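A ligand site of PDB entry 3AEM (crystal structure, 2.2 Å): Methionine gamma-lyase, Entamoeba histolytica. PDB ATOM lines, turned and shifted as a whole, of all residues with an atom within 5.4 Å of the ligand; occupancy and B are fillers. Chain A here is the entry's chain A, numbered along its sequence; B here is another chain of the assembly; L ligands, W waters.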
ATOM      1  N   SER A  82       0.991 -38.423 -15.488  1.00  0.00           N
ATOM      2  CA  SER A  82       0.614 -37.147 -16.087  1.00  0.00           C
ATOM      3  C   SER A  82       0.698 -37.276 -17.607  1.00  0.00           C
ATOM      4  O   SER A  82       1.339 -38.197 -18.093  1.00  0.00           O
ATOM      5  CB  SER A  82       1.548 -36.025 -15.602  1.00  0.00           C
ATOM      6  OG  SER A  82       2.886 -36.373 -15.909  1.00  0.00           O
ATOM      7  N   GLY A  83       0.056 -36.377 -18.347  1.00  0.00           N
ATOM      8  CA  GLY A  83       0.304 -36.243 -19.785  1.00  0.00           C
ATOM      9  C   GLY A  83       1.784 -36.094 -20.104  1.00  0.00           C
ATOM     10  O   GLY A  83       2.307 -36.712 -21.071  1.00  0.00           O
ATOM     11  N   MET A  84       2.488 -35.302 -19.294  1.00  0.00           N
ATOM     12  CA  MET A  84       3.917 -35.112 -19.523  1.00  0.00           C
ATOM     13  C   MET A  84       4.660 -36.441 -19.405  1.00  0.00           C
ATOM     14  O   MET A  84       5.606 -36.666 -20.151  1.00  0.00           O
ATOM     15  CB  MET A  84       4.558 -34.019 -18.598  1.00  0.00           C
ATOM     16  CG  MET A  84       4.153 -32.571 -18.955  1.00  0.00           C
ATOM     17  SD  MET A  84       4.037 -32.226 -20.762  1.00  0.00           S
ATOM     18  CE  MET A  84       5.739 -32.524 -21.297  1.00  0.00           C
ATOM     19  N   GLY A  85       4.207 -37.321 -18.488  1.00  0.00           N
ATOM     20  CA  GLY A  85       4.824 -38.630 -18.306  1.00  0.00           C
ATOM     21  C   GLY A  85       4.558 -39.467 -19.559  1.00  0.00           C
ATOM     22  O   GLY A  85       5.455 -40.192 -20.015  1.00  0.00           O
ATOM     23  N   ILE A  87       4.071 -38.214 -22.587  1.00  0.00           N
ATOM     24  CA  ILE A  87       4.872 -37.569 -23.661  1.00  0.00           C
ATOM     25  C   ILE A  87       6.379 -37.937 -23.612  1.00  0.00           C
ATOM     26  O   ILE A  87       6.947 -38.362 -24.633  1.00  0.00           O
ATOM     27  CB  ILE A  87       4.662 -36.050 -23.692  1.00  0.00           C
ATOM     28  CG1 ILE A  87       3.193 -35.762 -24.081  1.00  0.00           C
ATOM     29  CG2 ILE A  87       5.632 -35.363 -24.756  1.00  0.00           C
ATOM     30  CD1 ILE A  87       2.745 -34.333 -23.786  1.00  0.00           C
ATOM     31  N   TYR A 108       1.749 -27.447 -26.496  1.00  0.00           N
ATOM     32  CA  TYR A 108       1.673 -27.227 -25.059  1.00  0.00           C
ATOM     33  C   TYR A 108       3.044 -26.774 -24.476  1.00  0.00           C
ATOM     34  O   TYR A 108       4.096 -27.298 -24.836  1.00  0.00           O
ATOM     35  CB  TYR A 108       1.183 -28.521 -24.394  1.00  0.00           C
ATOM     36  CG  TYR A 108       1.129 -28.375 -22.905  1.00  0.00           C
ATOM     37  CD1 TYR A 108       0.291 -27.441 -22.328  1.00  0.00           C
ATOM     38  CD2 TYR A 108       1.946 -29.149 -22.080  1.00  0.00           C
ATOM     39  CE1 TYR A 108       0.252 -27.274 -20.949  1.00  0.00           C
ATOM     40  CE2 TYR A 108       1.911 -28.994 -20.695  1.00  0.00           C
ATOM     41  CZ  TYR A 108       1.061 -28.056 -20.133  1.00  0.00           C
ATOM     42  OH  TYR A 108       1.015 -27.865 -18.767  1.00  0.00           O
ATOM     43  N   CYS A 110       4.866 -27.057 -21.721  1.00  0.00           N
ATOM     44  CA  CYS A 110       5.842 -27.955 -21.096  1.00  0.00           C
ATOM     45  C   CYS A 110       6.351 -29.010 -22.091  1.00  0.00           C
ATOM     46  O   CYS A 110       7.403 -29.572 -21.904  1.00  0.00           O
ATOM     47  CB  CYS A 110       5.276 -28.597 -19.812  1.00  0.00           C
ATOM     48  SG  CYS A 110       4.806 -27.387 -18.552  1.00  0.00           S
ATOM     49  N   THR A 111       5.623 -29.257 -23.175  1.00  0.00           N
ATOM     50  CA  THR A 111       6.160 -30.081 -24.252  1.00  0.00           C
ATOM     51  C   THR A 111       7.281 -29.284 -24.971  1.00  0.00           C
ATOM     52  O   THR A 111       8.372 -29.819 -25.234  1.00  0.00           O
ATOM     53  CB  THR A 111       5.048 -30.450 -25.232  1.00  0.00           C
ATOM     54  OG1 THR A 111       4.022 -31.115 -24.496  1.00  0.00           O
ATOM     55  CG2 THR A 111       5.564 -31.346 -26.355  1.00  0.00           C
ATOM     56  N   GLU A 151       0.700 -32.158 -32.439  1.00  0.00           N
ATOM     57  CA  GLU A 151      -0.461 -31.875 -31.600  1.00  0.00           C
ATOM     58  C   GLU A 151      -1.399 -31.219 -32.588  1.00  0.00           C
ATOM     59  O   GLU A 151      -1.047 -30.201 -33.190  1.00  0.00           O
ATOM     60  CB  GLU A 151      -0.090 -30.796 -30.575  1.00  0.00           C
ATOM     61  CG  GLU A 151      -0.498 -31.011 -29.194  1.00  0.00           C
ATOM     62  CD  GLU A 151      -0.086 -29.852 -28.307  1.00  0.00           C
ATOM     63  OE1 GLU A 151      -0.869 -28.884 -28.178  1.00  0.00           O
ATOM     64  OE2 GLU A 151       1.019 -29.897 -27.719  1.00  0.00           O
ATOM     65  N   ASN A 155      -2.448 -26.717 -28.931  1.00  0.00           N
ATOM     66  CA  ASN A 155      -2.775 -25.968 -27.726  1.00  0.00           C
ATOM     67  C   ASN A 155      -1.839 -24.768 -27.699  1.00  0.00           C
ATOM     68  O   ASN A 155      -0.619 -24.975 -27.678  1.00  0.00           O
ATOM     69  CB  ASN A 155      -2.545 -26.862 -26.522  1.00  0.00           C
ATOM     70  CG  ASN A 155      -2.885 -26.208 -25.192  1.00  0.00           C
ATOM     71  OD1 ASN A 155      -3.132 -25.005 -25.108  1.00  0.00           O
ATOM     72  ND2 ASN A 155      -2.920 -27.015 -24.122  1.00  0.00           N
ATOM     73  N   ASP A 180      -0.350 -36.118 -30.089  1.00  0.00           N
ATOM     74  CA  ASP A 180      -1.009 -35.732 -28.840  1.00  0.00           C
ATOM     75  C   ASP A 180      -2.437 -35.299 -29.217  1.00  0.00           C
ATOM     76  O   ASP A 180      -2.635 -34.258 -29.829  1.00  0.00           O
ATOM     77  CB  ASP A 180      -0.229 -34.620 -28.161  1.00  0.00           C
ATOM     78  CG  ASP A 180      -0.837 -34.203 -26.838  1.00  0.00           C
ATOM     79  OD1 ASP A 180      -2.017 -34.580 -26.559  1.00  0.00           O
ATOM     80  OD2 ASP A 180      -0.110 -33.492 -26.082  1.00  0.00           O
ATOM     81  N   THR A 182      -4.998 -34.869 -27.018  1.00  0.00           N
ATOM     82  CA  THR A 182      -5.599 -34.370 -25.793  1.00  0.00           C
ATOM     83  C   THR A 182      -6.780 -33.416 -26.074  1.00  0.00           C
ATOM     84  O   THR A 182      -7.849 -33.542 -25.442  1.00  0.00           O
ATOM     85  CB  THR A 182      -4.539 -33.610 -24.955  1.00  0.00           C
ATOM     86  OG1 THR A 182      -3.511 -34.528 -24.518  1.00  0.00           O
ATOM     87  CG2 THR A 182      -5.159 -32.919 -23.736  1.00  0.00           C
ATOM     88  N   PHE A 183      -6.605 -32.490 -27.023  1.00  0.00           N
ATOM     89  CA  PHE A 183      -7.558 -31.363 -27.208  1.00  0.00           C
ATOM     90  C   PHE A 183      -8.887 -31.794 -27.791  1.00  0.00           C
ATOM     91  O   PHE A 183      -9.894 -31.080 -27.708  1.00  0.00           O
ATOM     92  CB  PHE A 183      -6.941 -30.284 -28.114  1.00  0.00           C
ATOM     93  CG  PHE A 183      -6.733 -28.938 -27.442  1.00  0.00           C
ATOM     94  CD1 PHE A 183      -6.163 -28.851 -26.194  1.00  0.00           C
ATOM     95  CD2 PHE A 183      -7.023 -27.764 -28.126  1.00  0.00           C
ATOM     96  CE1 PHE A 183      -5.899 -27.629 -25.628  1.00  0.00           C
ATOM     97  CE2 PHE A 183      -6.787 -26.526 -27.547  1.00  0.00           C
ATOM     98  CZ  PHE A 183      -6.239 -26.467 -26.290  1.00  0.00           C
ATOM     99  N   SER A 202      -3.159 -36.224 -22.416  1.00  0.00           N
ATOM    100  CA  SER A 202      -3.318 -35.863 -21.041  1.00  0.00           C
ATOM    101  C   SER A 202      -4.730 -36.298 -20.626  1.00  0.00           C
ATOM    102  O   SER A 202      -5.721 -35.693 -21.016  1.00  0.00           O
ATOM    103  CB  SER A 202      -3.129 -34.381 -20.846  1.00  0.00           C
ATOM    104  OG  SER A 202      -3.449 -34.040 -19.522  1.00  0.00           O
ATOM    105  N   VAL A 203      -4.804 -37.344 -19.805  1.00  0.00           N
ATOM    106  CA  VAL A 203      -6.065 -37.850 -19.255  1.00  0.00           C
ATOM    107  C   VAL A 203      -6.630 -36.845 -18.257  1.00  0.00           C
ATOM    108  O   VAL A 203      -7.810 -36.852 -17.957  1.00  0.00           O
ATOM    109  CB  VAL A 203      -5.773 -39.216 -18.605  1.00  0.00           C
ATOM    110  CG1 VAL A 203      -6.991 -39.758 -17.853  1.00  0.00           C
ATOM    111  CG2 VAL A 203      -5.372 -40.191 -19.714  1.00  0.00           C
ATOM    112  N   SER A 204      -5.769 -35.943 -17.781  1.00  0.00           N
ATOM    113  CA  SER A 204      -6.145 -34.842 -16.900  1.00  0.00           C
ATOM    114  C   SER A 204      -7.231 -33.954 -17.483  1.00  0.00           C
ATOM    115  O   SER A 204      -7.956 -33.273 -16.744  1.00  0.00           O
ATOM    116  CB  SER A 204      -4.928 -33.952 -16.638  1.00  0.00           C
ATOM    117  OG  SER A 204      -3.746 -34.715 -16.481  1.00  0.00           O
ATOM    118  N   LYS A 205      -7.371 -33.985 -18.800  1.00  0.00           N
ATOM    119  CA  LYS A 205      -8.354 -33.132 -19.460  1.00  0.00           C
ATOM    120  C   LYS A 205      -9.683 -33.889 -19.673  1.00  0.00           C
ATOM    121  O   LYS A 205     -10.284 -34.320 -18.689  1.00  0.00           O
ATOM    122  CB  LYS A 205      -7.784 -32.532 -20.747  1.00  0.00           C
ATOM    123  CG  LYS A 205      -6.381 -31.974 -20.650  1.00  0.00           C
ATOM    124  CD  LYS A 205      -6.129 -31.121 -19.419  1.00  0.00           C
ATOM    125  CE  LYS A 205      -4.788 -30.498 -19.567  1.00  0.00           C
ATOM    126  NZ  LYS A 205      -4.481 -29.911 -18.290  1.00  0.00           N
ATOM    127  N   ILE A 214      -4.628 -35.794 -12.201  1.00  0.00           N
ATOM    128  CA  ILE A 214      -3.599 -35.601 -13.211  1.00  0.00           C
ATOM    129  C   ILE A 214      -3.171 -36.989 -13.712  1.00  0.00           C
ATOM    130  O   ILE A 214      -2.851 -37.864 -12.910  1.00  0.00           O
ATOM    131  CB  ILE A 214      -2.373 -34.845 -12.645  1.00  0.00           C
ATOM    132  CG1 ILE A 214      -2.792 -33.477 -12.080  1.00  0.00           C
ATOM    133  CG2 ILE A 214      -1.295 -34.687 -13.717  1.00  0.00           C
ATOM    134  CD1 ILE A 214      -3.131 -32.429 -13.075  1.00  0.00           C
ATOM    135  N   GLY A 215      -3.184 -37.215 -15.017  1.00  0.00           N
ATOM    136  CA  GLY A 215      -2.723 -38.498 -15.511  1.00  0.00           C
ATOM    137  C   GLY A 215      -2.455 -38.424 -16.995  1.00  0.00           C
ATOM    138  O   GLY A 215      -2.837 -37.454 -17.617  1.00  0.00           O
ATOM    139  N   GLY A 216      -1.819 -39.451 -17.535  1.00  0.00           N
ATOM    140  CA  GLY A 216      -1.591 -39.543 -18.947  1.00  0.00           C
ATOM    141  C   GLY A 216      -1.780 -40.939 -19.506  1.00  0.00           C
ATOM    142  O   GLY A 216      -1.801 -41.933 -18.788  1.00  0.00           O
ATOM    143  N   VAL A 331      -6.121 -22.333 -15.280  1.00  0.00           N
ATOM    144  CA  VAL A 331      -5.535 -23.114 -16.383  1.00  0.00           C
ATOM    145  C   VAL A 331      -6.141 -24.538 -16.368  1.00  0.00           C
ATOM    146  O   VAL A 331      -6.959 -24.854 -15.493  1.00  0.00           O
ATOM    147  CB  VAL A 331      -3.965 -23.134 -16.342  1.00  0.00           C
ATOM    148  CG1 VAL A 331      -3.403 -21.700 -16.268  1.00  0.00           C
ATOM    149  CG2 VAL A 331      -3.455 -23.973 -15.183  1.00  0.00           C
ATOM    150  N   SER A 332      -5.725 -25.358 -17.339  1.00  0.00           N
ATOM    151  CA  SER A 332      -6.292 -26.674 -17.595  1.00  0.00           C
ATOM    152  C   SER A 332      -7.530 -26.553 -18.471  1.00  0.00           C
ATOM    153  O   SER A 332      -7.972 -25.446 -18.837  1.00  0.00           O
ATOM    154  CB  SER A 332      -6.593 -27.429 -16.302  1.00  0.00           C
ATOM    155  OG  SER A 332      -6.740 -28.791 -16.624  1.00  0.00           O
ATOM    156  N   LEU A 333      -8.116 -27.687 -18.827  1.00  0.00           N
ATOM    157  CA  LEU A 333      -9.219 -27.655 -19.810  1.00  0.00           C
ATOM    158  C   LEU A 333      -9.910 -29.008 -19.799  1.00  0.00           C
ATOM    159  O   LEU A 333      -9.419 -29.966 -19.141  1.00  0.00           O
ATOM    160  CB  LEU A 333      -8.668 -27.345 -21.221  1.00  0.00           C
ATOM    161  CG  LEU A 333      -7.613 -28.356 -21.742  1.00  0.00           C
ATOM    162  CD1 LEU A 333      -8.107 -29.154 -22.977  1.00  0.00           C
ATOM    163  CD2 LEU A 333      -6.287 -27.664 -22.079  1.00  0.00           C
ATOM    164  N   GLU A 341      -8.625 -18.753 -19.466  1.00  0.00           N
ATOM    165  CA  GLU A 341      -7.259 -18.322 -19.107  1.00  0.00           C
ATOM    166  C   GLU A 341      -6.633 -17.440 -20.195  1.00  0.00           C
ATOM    167  O   GLU A 341      -7.151 -17.308 -21.301  1.00  0.00           O
ATOM    168  CB  GLU A 341      -6.335 -19.520 -18.803  1.00  0.00           C
ATOM    169  CG  GLU A 341      -6.080 -20.503 -19.997  1.00  0.00           C
ATOM    170  CD  GLU A 341      -4.679 -20.413 -20.611  1.00  0.00           C
ATOM    171  OE1 GLU A 341      -4.424 -21.008 -21.688  1.00  0.00           O
ATOM    172  OE2 GLU A 341      -3.802 -19.757 -20.014  1.00  0.00           O
ATOM    173  N   MET A 346       0.133 -17.020 -18.726  1.00  0.00           N
ATOM    174  CA  MET A 346      -0.159 -18.229 -17.941  1.00  0.00           C
ATOM    175  C   MET A 346       0.377 -19.540 -18.593  1.00  0.00           C
ATOM    176  O   MET A 346       1.528 -19.890 -18.379  1.00  0.00           O
ATOM    177  CB  MET A 346      -1.679 -18.313 -17.570  1.00  0.00           C
ATOM    178  CG  MET A 346      -2.295 -17.071 -16.799  1.00  0.00           C
ATOM    179  SD  MET A 346      -4.135 -17.169 -16.485  1.00  0.00           S
ATOM    180  CE  MET A 346      -4.446 -15.603 -15.722  1.00  0.00           C
ATOM    181  N   THR A 347      -0.420 -20.275 -19.367  1.00  0.00           N
ATOM    182  CA  THR A 347       0.000 -21.608 -19.871  1.00  0.00           C
ATOM    183  C   THR A 347       1.201 -21.610 -20.799  1.00  0.00           C
ATOM    184  O   THR A 347       1.916 -22.605 -20.911  1.00  0.00           O
ATOM    185  CB  THR A 347      -1.128 -22.389 -20.584  1.00  0.00           C
ATOM    186  OG1 THR A 347      -1.646 -21.617 -21.693  1.00  0.00           O
ATOM    187  CG2 THR A 347      -2.226 -22.798 -19.625  1.00  0.00           C
ATOM    188  N   ARG A 367      -8.126 -17.948 -24.001  1.00  0.00           N
ATOM    189  CA  ARG A 367      -8.502 -19.335 -24.282  1.00  0.00           C
ATOM    190  C   ARG A 367      -9.642 -19.759 -23.373  1.00  0.00           C
ATOM    191  O   ARG A 367      -9.611 -19.525 -22.158  1.00  0.00           O
ATOM    192  CB  ARG A 367      -7.317 -20.319 -24.104  1.00  0.00           C
ATOM    193  CG  ARG A 367      -7.568 -21.732 -24.737  1.00  0.00           C
ATOM    194  CD  ARG A 367      -6.539 -22.787 -24.277  1.00  0.00           C
ATOM    195  NE  ARG A 367      -6.720 -23.140 -22.866  1.00  0.00           N
ATOM    196  CZ  ARG A 367      -5.813 -23.797 -22.141  1.00  0.00           C
ATOM    197  NH1 ARG A 367      -4.660 -24.189 -22.669  1.00  0.00           N
ATOM    198  NH2 ARG A 367      -6.072 -24.044 -20.858  1.00  0.00           N
ATOM    199  N   PHE B  44       2.751 -17.762 -11.918  1.00  0.00           N
ATOM    200  CA  PHE B  44       3.552 -18.336 -12.995  1.00  0.00           C
ATOM    201  C   PHE B  44       4.982 -17.764 -13.058  1.00  0.00           C
ATOM    202  O   PHE B  44       5.871 -18.368 -13.640  1.00  0.00           O
ATOM    203  CB  PHE B  44       2.864 -18.136 -14.338  1.00  0.00           C
ATOM    204  CG  PHE B  44       1.979 -19.290 -14.741  1.00  0.00           C
ATOM    205  CD1 PHE B  44       0.598 -19.229 -14.539  1.00  0.00           C
ATOM    206  CD2 PHE B  44       2.535 -20.441 -15.296  1.00  0.00           C
ATOM    207  CE1 PHE B  44      -0.216 -20.280 -14.901  1.00  0.00           C
ATOM    208  CE2 PHE B  44       1.731 -21.515 -15.660  1.00  0.00           C
ATOM    209  CZ  PHE B  44       0.352 -21.445 -15.456  1.00  0.00           C
ATOM    210  N   ILE B  52      -1.235 -23.400  -8.672  1.00  0.00           N
ATOM    211  CA  ILE B  52      -1.664 -23.224 -10.042  1.00  0.00           C
ATOM    212  C   ILE B  52      -2.268 -24.540 -10.567  1.00  0.00           C
ATOM    213  O   ILE B  52      -3.364 -24.549 -11.152  1.00  0.00           O
ATOM    214  CB  ILE B  52      -0.429 -22.847 -10.922  1.00  0.00           C
ATOM    215  CG1 ILE B  52       0.237 -21.531 -10.431  1.00  0.00           C
ATOM    216  CG2 ILE B  52      -0.817 -22.814 -12.379  1.00  0.00           C
ATOM    217  CD1 ILE B  52       1.586 -21.197 -11.165  1.00  0.00           C
ATOM    218  N   TYR B  53      -1.507 -25.630 -10.417  1.00  0.00           N
ATOM    219  CA  TYR B  53      -1.820 -26.876 -11.121  1.00  0.00           C
ATOM    220  C   TYR B  53      -1.036 -27.967 -10.431  1.00  0.00           C
ATOM    221  O   TYR B  53       0.143 -27.757 -10.110  1.00  0.00           O
ATOM    222  CB  TYR B  53      -1.388 -26.749 -12.586  1.00  0.00           C
ATOM    223  CG  TYR B  53      -1.798 -27.899 -13.472  1.00  0.00           C
ATOM    224  CD1 TYR B  53      -3.171 -28.126 -13.791  1.00  0.00           C
ATOM    225  CD2 TYR B  53      -0.838 -28.731 -14.010  1.00  0.00           C
ATOM    226  CE1 TYR B  53      -3.537 -29.190 -14.620  1.00  0.00           C
ATOM    227  CE2 TYR B  53      -1.191 -29.776 -14.843  1.00  0.00           C
ATOM    228  CZ  TYR B  53      -2.537 -30.002 -15.144  1.00  0.00           C
ATOM    229  OH  TYR B  53      -2.839 -31.062 -15.943  1.00  0.00           O
ATOM    230  N   ARG B  55       0.485 -30.711 -11.067  1.00  0.00           N
ATOM    231  CA  ARG B  55       1.806 -31.114 -11.560  1.00  0.00           C
ATOM    232  C   ARG B  55       2.914 -30.118 -11.129  1.00  0.00           C
ATOM    233  O   ARG B  55       4.037 -30.538 -10.876  1.00  0.00           O
ATOM    234  CB  ARG B  55       1.843 -31.355 -13.089  1.00  0.00           C
ATOM    235  CG  ARG B  55       3.285 -31.652 -13.657  1.00  0.00           C
ATOM    236  CD  ARG B  55       3.268 -32.363 -15.052  1.00  0.00           C
ATOM    237  NE  ARG B  55       2.361 -31.701 -15.971  1.00  0.00           N
ATOM    238  CZ  ARG B  55       2.525 -30.484 -16.499  1.00  0.00           C
ATOM    239  NH1 ARG B  55       3.655 -29.773 -16.301  1.00  0.00           N
ATOM    240  NH2 ARG B  55       1.573 -30.015 -17.284  1.00  0.00           N
ATOM    241  N   LEU B  56       2.601 -28.820 -11.030  1.00  0.00           N
ATOM    242  CA  LEU B  56       3.580 -27.844 -10.532  1.00  0.00           C
ATOM    243  C   LEU B  56       3.627 -27.891  -8.998  1.00  0.00           C
ATOM    244  O   LEU B  56       4.632 -27.553  -8.401  1.00  0.00           O
ATOM    245  CB  LEU B  56       3.250 -26.408 -11.002  1.00  0.00           C
ATOM    246  CG  LEU B  56       3.045 -26.214 -12.513  1.00  0.00           C
ATOM    247  CD1 LEU B  56       2.736 -24.760 -12.929  1.00  0.00           C
ATOM    248  CD2 LEU B  56       4.245 -26.700 -13.288  1.00  0.00           C
HETATM  249  C1  LIG L   1      -3.068 -26.336 -20.036  1.00  0.00           C
HETATM  250  N1  LIG L   1      -2.194 -28.584 -20.413  1.00  0.00           N
HETATM  251  O1  LIG L   1      -3.832 -25.675 -19.390  1.00  0.00           O
HETATM  252  P1  LIG L   1      -0.458 -33.075 -17.880  1.00  0.00           P
HETATM  253  N2  LIG L   1      -0.669 -32.144 -23.869  1.00  0.00           N
HETATM  254  C2  LIG L   1      -1.590 -31.165 -23.993  1.00  0.00           C
HETATM  255  C3  LIG L   1      -1.981 -30.412 -22.867  1.00  0.00           C
HETATM  256  O2  LIG L   1      -2.903 -29.435 -23.056  1.00  0.00           O
HETATM  257  C4  LIG L   1      -1.494 -30.684 -21.571  1.00  0.00           C
HETATM  258  C5  LIG L   1      -0.507 -31.660 -21.510  1.00  0.00           C
HETATM  259  C6  LIG L   1      -0.160 -32.390 -22.660  1.00  0.00           C
HETATM  260  C7  LIG L   1      -2.455 -27.557 -19.474  1.00  0.00           C
HETATM  261  C8  LIG L   1      -2.074 -27.572 -17.980  1.00  0.00           C
HETATM  262  S1  LIG L   1      -0.234 -25.430 -16.888  1.00  0.00           S
HETATM  263  C9  LIG L   1       0.934 -24.660 -17.975  1.00  0.00           C
HETATM  264  C10 LIG L   1      -1.739 -26.067 -17.657  1.00  0.00           C
HETATM  265  C11 LIG L   1      -2.180 -30.901 -25.367  1.00  0.00           C
HETATM  266  C12 LIG L   1      -1.746 -29.829 -20.354  1.00  0.00           C
HETATM  267  C13 LIG L   1       0.193 -32.029 -20.239  1.00  0.00           C
HETATM  268  O3  LIG L   1      -1.462 -34.143 -17.517  1.00  0.00           O
HETATM  269  O4  LIG L   1      -0.900 -31.699 -17.425  1.00  0.00           O
HETATM  270  O5  LIG L   1       0.960 -33.433 -17.590  1.00  0.00           O
HETATM  271  O6  LIG L   1      -0.607 -32.933 -19.490  1.00  0.00           O
HETATM  272  O7  LIG L   1      -2.882 -25.944 -21.192  1.00  0.00           O
HETATM  273  O   HOH W   1      -1.483 -23.984 -22.881  1.00  0.00           O
HETATM  274  O   HOH W   2      -3.439 -29.731 -28.394  1.00  0.00           O
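Ser 82 touches the ligand. Ile 87 touches the ligand. Glu 151 touches the ligand (OE1 to C11, 3.7 Å). Thr 182 touches the ligand (CB to C11, 3.6 Å). Ile 214 touches the ligand. Gly 215 touches the ligand. Val 331 touches the ligand (CG2 to C10, 3.7 Å). CD2 of Leu 333 touches O7 of the ligand, 3.9 Å away. Thr 347 touches the ligand (CG2 to O1, 3.3 Å). Phe 44 of chain B touches the ligand. Hydrophobic or aromatic side chains that line the ligand: Met 84, Ile 87, Tyr 108, Ile 214, Val 331, Leu 333, Phe 44 of chain B and Tyr 53 of chain B. Of the 32 residues printed, 22 come within 4 Å of the ligand. The nearest printed residue that does not touch the ligand is Phe 183 (4.3 Å).
An oxygen (O4) of the ligand sits at hydrogen-bond distance from the side-chain hydroxyl (OH) of Tyr 53 of chain B (2.5 Å). The backbone NH of Gly 83 is in hydrogen-bond range of an oxygen (O3) of the ligand, 2.8 Å away. The guanidinium group of Arg 367 lies within salt-bridge range of an oxygen (O7) of the ligand (2.9 Å). ND2 of Asn 155 sits at hydrogen-bond distance from O2 of the ligand. O3 of the ligand sits at hydrogen-bond distance from OG of Ser 202, 2.8 Å away. The backbone NH (N) of Met 84 lies within hydrogen-bond range of an oxygen (O5) of the ligand. The backbone NH of Ser 332 is in hydrogen-bond range of an oxygen (O1) of the ligand (2.8 Å). The side-chain hydroxyl (OG) of Ser 204 lies within hydrogen-bond range of an oxygen (O3) of the ligand (2.6 Å). The side-chain carboxylate of Asp 180 sits at hydrogen-bond distance from a nitrogen (N2) of the ligand (2.7 Å). NZ of Lys 205 lies close to N1 of the ligand, 3.4 Å away. OH of Tyr 108 lies close to S1 of the ligand (3.3 Å). O5 of the ligand lies within salt-bridge range of NE of Arg 55 of chain B.
Water W1 lies within hydrogen-bond range of the side-chain hydroxyl (OG1) of Thr 347, an oxygen (O7) of the ligand, the side-chain amide oxygen (OD1) of Asn 155 and the guanidinium group (NH1) of Arg 367. Water W2 lies within hydrogen-bond range of OE1 of Glu 151 and N of Asn 155.
The backbone NH of Tyr 108 sits at hydrogen-bond distance from the side-chain carboxylate of Glu 151 (2.8 Å). The side-chain hydroxyl (OG) of Ser 204 is in hydrogen-bond range of the backbone NH (N) of Gly 215 (3.0 Å). The backbone NH (N) of Ser 202 sits at hydrogen-bond distance from the side-chain hydroxyl (OG1) of Thr 182 (2.7 Å). NH1 of Arg 367 is in salt-bridge range of OE1 of Glu 341 (3.3 Å). The side-chain hydroxyl (OG1) of Thr 347 is in hydrogen-bond range of the side-chain carboxylate (OE1) of Glu 341 (2.8 Å). N of Val 203 sits at hydrogen-bond distance from O of Gly 215 (2.9 Å). The side-chain amide oxygen of Asn 155 lies within hydrogen-bond range of the guanidinium group of Arg 367, at 3.0 Å. O of Ser 82 lies close to N of Gly 216 (3.4 Å).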
